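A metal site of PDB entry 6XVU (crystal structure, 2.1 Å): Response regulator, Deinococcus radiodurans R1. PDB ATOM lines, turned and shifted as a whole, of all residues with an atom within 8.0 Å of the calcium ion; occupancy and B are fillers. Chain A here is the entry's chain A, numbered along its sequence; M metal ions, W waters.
Glu 29 touches the calcium ion.
Four residues have an atom within 4 Å of the calcium ion: Glu 29, Asp 30, Asp 80 and Asn 82.
The nearest printed residue that does not touch the calcium ion is Met 83 (4.5 Å).
Water W2 binds the calcium ion.
The calcium ion is bound by water W3, 2.2 Å away.
The side-chain carboxylate (OD2) of Asp 80 is bound to the calcium ion (2.3 Å).
The calcium ion is bound by O of Asn 82, at 2.3 Å.
The side-chain carboxylate (OD1) of Asp 30 binds the calcium ion (2.4 Å).
Water W1 is bound to the calcium ion (2.5 Å).
The side-chain amino group of Lys 132 lies within salt-bridge range of the side-chain carboxylate of Glu 29 (2.8 Å).
The guanidinium group of Arg 55 sits at hydrogen-bond distance from the backbone carbonyl oxygen of Asp 30.
NE of Arg 55 sits close to O of Glu 29 (3.4 Å).
The side-chain amino group of Lys 132 is in salt-bridge range of the side-chain carboxylate of Asp 80.
N of Asp 80 sits at hydrogen-bond distance from O of Val 28 (3.1 Å).
The side-chain carboxylate of Glu 29 lies within hydrogen-bond range of the backbone NH of Asn 31.
OD1 of Asp 80 sits at hydrogen-bond distance from OG1 of Thr 110.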
ATOM      1  N   VAL A  28      -3.322  21.710   8.910  1.00  0.00           N
ATOM      2  CA  VAL A  28      -2.395  21.065   7.930  1.00  0.00           C
ATOM      3  C   VAL A  28      -1.070  20.885   8.639  1.00  0.00           C
ATOM      4  O   VAL A  28      -0.405  21.872   8.947  1.00  0.00           O
ATOM      5  CB  VAL A  28      -2.235  21.842   6.620  1.00  0.00           C
ATOM      6  CG1 VAL A  28      -1.586  21.004   5.530  1.00  0.00           C
ATOM      7  CG2 VAL A  28      -3.568  22.412   6.123  1.00  0.00           C
ATOM      8  N   GLU A  29      -0.769  19.661   8.985  1.00  0.00           N
ATOM      9  CA  GLU A  29       0.343  19.301   9.895  1.00  0.00           C
ATOM     10  C   GLU A  29       0.734  17.862   9.617  1.00  0.00           C
ATOM     11  O   GLU A  29      -0.188  17.028   9.493  1.00  0.00           O
ATOM     12  CB  GLU A  29      -0.139  19.515  11.324  1.00  0.00           C
ATOM     13  CG  GLU A  29       0.825  18.984  12.378  1.00  0.00           C
ATOM     14  CD  GLU A  29       2.175  19.666  12.371  1.00  0.00           C
ATOM     15  OE1 GLU A  29       2.232  20.864  12.722  1.00  0.00           O
ATOM     16  OE2 GLU A  29       3.185  18.976  12.015  1.00  0.00           O
ATOM     17  N   ASP A  30       2.032  17.588   9.461  1.00  0.00           N
ATOM     18  CA  ASP A  30       2.568  16.252   9.151  1.00  0.00           C
ATOM     19  C   ASP A  30       2.825  15.447  10.442  1.00  0.00           C
ATOM     20  O   ASP A  30       2.689  14.247  10.402  1.00  0.00           O
ATOM     21  CB  ASP A  30       3.815  16.370   8.277  1.00  0.00           C
ATOM     22  CG  ASP A  30       4.948  17.215   8.863  1.00  0.00           C
ATOM     23  OD1 ASP A  30       4.655  18.209   9.514  1.00  0.00           O
ATOM     24  OD2 ASP A  30       6.137  16.836   8.696  1.00  0.00           O
ATOM     25  N   ASN A  31       3.144  16.110  11.556  1.00  0.00           N
ATOM     26  CA  ASN A  31       3.516  15.421  12.807  1.00  0.00           C
ATOM     27  C   ASN A  31       2.263  15.131  13.667  1.00  0.00           C
ATOM     28  O   ASN A  31       1.539  16.061  14.090  1.00  0.00           O
ATOM     29  CB  ASN A  31       4.613  16.189  13.542  1.00  0.00           C
ATOM     30  CG  ASN A  31       5.182  15.286  14.627  1.00  0.00           C
ATOM     31  OD1 ASN A  31       5.573  14.137  14.371  1.00  0.00           O
ATOM     32  ND2 ASN A  31       5.185  15.782  15.847  1.00  0.00           N
ATOM     33  N   ASP A  34       1.719  16.970  17.029  1.00  0.00           N
ATOM     34  CA  ASP A  34       1.219  18.368  16.896  1.00  0.00           C
ATOM     35  C   ASP A  34      -0.310  18.334  16.701  1.00  0.00           C
ATOM     36  O   ASP A  34      -1.021  19.212  17.212  1.00  0.00           O
ATOM     37  CB  ASP A  34       1.966  19.086  15.785  1.00  0.00           C
ATOM     38  CG  ASP A  34       3.451  19.369  16.031  1.00  0.00           C
ATOM     39  OD1 ASP A  34       4.296  18.462  15.826  1.00  0.00           O
ATOM     40  OD2 ASP A  34       3.771  20.491  16.412  1.00  0.00           O
ATOM     41  N   ARG A  55      -2.543  16.069   6.263  1.00  0.00           N
ATOM     42  CA  ARG A  55      -1.142  15.733   6.666  1.00  0.00           C
ATOM     43  C   ARG A  55      -0.117  16.462   5.795  1.00  0.00           C
ATOM     44  O   ARG A  55       1.047  16.442   6.140  1.00  0.00           O
ATOM     45  CB  ARG A  55      -0.926  14.228   6.587  1.00  0.00           C
ATOM     46  CG  ARG A  55      -1.735  13.416   7.606  1.00  0.00           C
ATOM     47  CD  ARG A  55      -1.892  13.985   9.010  1.00  0.00           C
ATOM     48  NE  ARG A  55      -0.671  13.702   9.768  1.00  0.00           N
ATOM     49  CZ  ARG A  55      -0.397  12.544  10.409  1.00  0.00           C
ATOM     50  NH1 ARG A  55      -1.254  11.539  10.450  1.00  0.00           N
ATOM     51  NH2 ARG A  55       0.758  12.374  11.005  1.00  0.00           N
ATOM     52  N   ASP A  80       1.453  24.349   8.804  1.00  0.00           N
ATOM     53  CA  ASP A  80       2.900  24.282   9.084  1.00  0.00           C
ATOM     54  C   ASP A  80       3.668  24.580   7.792  1.00  0.00           C
ATOM     55  O   ASP A  80       3.037  24.561   6.723  1.00  0.00           O
ATOM     56  CB  ASP A  80       3.127  22.924   9.716  1.00  0.00           C
ATOM     57  CG  ASP A  80       4.550  22.665  10.106  1.00  0.00           C
ATOM     58  OD1 ASP A  80       5.161  23.558  10.769  1.00  0.00           O
ATOM     59  OD2 ASP A  80       5.043  21.678   9.548  1.00  0.00           O
ATOM     60  N   LEU A  81       4.913  24.967   7.888  1.00  0.00           N
ATOM     61  CA  LEU A  81       5.740  25.350   6.704  1.00  0.00           C
ATOM     62  C   LEU A  81       6.377  24.087   6.124  1.00  0.00           C
ATOM     63  O   LEU A  81       6.218  23.827   4.937  1.00  0.00           O
ATOM     64  CB  LEU A  81       6.801  26.371   7.128  1.00  0.00           C
ATOM     65  CG  LEU A  81       6.244  27.752   7.483  1.00  0.00           C
ATOM     66  CD1 LEU A  81       7.386  28.736   7.700  1.00  0.00           C
ATOM     67  CD2 LEU A  81       5.236  28.258   6.457  1.00  0.00           C
ATOM     68  N   ASN A  82       7.057  23.320   6.963  1.00  0.00           N
ATOM     69  CA  ASN A  82       7.881  22.180   6.515  1.00  0.00           C
ATOM     70  C   ASN A  82       7.013  20.920   6.541  1.00  0.00           C
ATOM     71  O   ASN A  82       6.787  20.384   7.644  1.00  0.00           O
ATOM     72  CB  ASN A  82       9.166  22.032   7.318  1.00  0.00           C
ATOM     73  CG  ASN A  82      10.040  20.983   6.684  1.00  0.00           C
ATOM     74  OD1 ASN A  82       9.788  20.576   5.556  1.00  0.00           O
ATOM     75  ND2 ASN A  82      11.029  20.510   7.406  1.00  0.00           N
ATOM     76  N   MET A  83       6.507  20.514   5.376  1.00  0.00           N
ATOM     77  CA  MET A  83       5.585  19.359   5.214  1.00  0.00           C
ATOM     78  C   MET A  83       5.939  18.693   3.914  1.00  0.00           C
ATOM     79  O   MET A  83       6.316  19.376   2.975  1.00  0.00           O
ATOM     80  CB  MET A  83       4.116  19.783   5.126  1.00  0.00           C
ATOM     81  CG  MET A  83       3.637  20.536   6.336  1.00  0.00           C
ATOM     82  SD  MET A  83       1.858  20.847   6.236  1.00  0.00           S
ATOM     83  CE  MET A  83       1.843  22.087   4.921  1.00  0.00           C
ATOM     84  N   PRO A  84       5.821  17.359   3.814  1.00  0.00           N
ATOM     85  CA  PRO A  84       6.192  16.693   2.584  1.00  0.00           C
ATOM     86  C   PRO A  84       5.219  17.005   1.433  1.00  0.00           C
ATOM     87  O   PRO A  84       4.100  17.370   1.669  1.00  0.00           O
ATOM     88  CB  PRO A  84       6.229  15.203   3.010  1.00  0.00           C
ATOM     89  CG  PRO A  84       5.243  15.106   4.128  1.00  0.00           C
ATOM     90  CD  PRO A  84       5.304  16.447   4.843  1.00  0.00           C
ATOM     91  N   LEU A 109       1.161  28.194  11.457  1.00  0.00           N
ATOM     92  CA  LEU A 109       1.523  27.796  12.832  1.00  0.00           C
ATOM     93  C   LEU A 109       2.679  26.829  12.706  1.00  0.00           C
ATOM     94  O   LEU A 109       2.464  25.708  12.209  1.00  0.00           O
ATOM     95  CB  LEU A 109       0.300  27.170  13.523  1.00  0.00           C
ATOM     96  CG  LEU A 109       0.571  26.527  14.880  1.00  0.00           C
ATOM     97  CD1 LEU A 109       0.950  27.568  15.887  1.00  0.00           C
ATOM     98  CD2 LEU A 109      -0.640  25.723  15.315  1.00  0.00           C
ATOM     99  N   THR A 110       3.875  27.258  13.117  1.00  0.00           N
ATOM    100  CA  THR A 110       5.129  26.591  12.753  1.00  0.00           C
ATOM    101  C   THR A 110       6.172  26.821  13.841  1.00  0.00           C
ATOM    102  O   THR A 110       6.047  27.818  14.613  1.00  0.00           O
ATOM    103  CB  THR A 110       5.516  27.128  11.369  1.00  0.00           C
ATOM    104  OG1 THR A 110       6.258  26.101  10.689  1.00  0.00           O
ATOM    105  CG2 THR A 110       6.123  28.532  11.431  1.00  0.00           C
ATOM    106  N   THR A 111       7.208  25.981  13.921  1.00  0.00           N
ATOM    107  CA  THR A 111       8.230  26.140  15.013  1.00  0.00           C
ATOM    108  C   THR A 111       9.286  27.206  14.592  1.00  0.00           C
ATOM    109  O   THR A 111       9.837  27.866  15.477  1.00  0.00           O
ATOM    110  CB  THR A 111       8.926  24.838  15.425  1.00  0.00           C
ATOM    111  OG1 THR A 111       9.553  24.395  14.239  1.00  0.00           O
ATOM    112  CG2 THR A 111       8.074  23.723  16.000  1.00  0.00           C
ATOM    113  N   LYS A 132       4.930  28.182  17.135  1.00  0.00           N
ATOM    114  CA  LYS A 132       4.713  27.169  18.208  1.00  0.00           C
ATOM    115  C   LYS A 132       5.608  27.491  19.388  1.00  0.00           C
ATOM    116  O   LYS A 132       6.800  27.640  19.269  1.00  0.00           O
ATOM    117  CB  LYS A 132       4.997  25.757  17.683  1.00  0.00           C
ATOM    118  CG  LYS A 132       3.981  25.290  16.640  1.00  0.00           C
ATOM    119  CD  LYS A 132       4.370  23.955  16.041  1.00  0.00           C
ATOM    120  CE  LYS A 132       3.487  23.518  14.914  1.00  0.00           C
ATOM    121  NZ  LYS A 132       4.067  22.372  14.198  1.00  0.00           N
HETATM  122 CA    CA M   1       6.364  19.833   9.874  1.00  0.00          CA
HETATM  123  O   HOH W   1       8.173  18.239   9.322  1.00  0.00           O
HETATM  124  O   HOH W   2       8.030  21.039  10.608  1.00  0.00           O
HETATM  125  O   HOH W   3       5.479  19.787  11.922  1.00  0.00           O
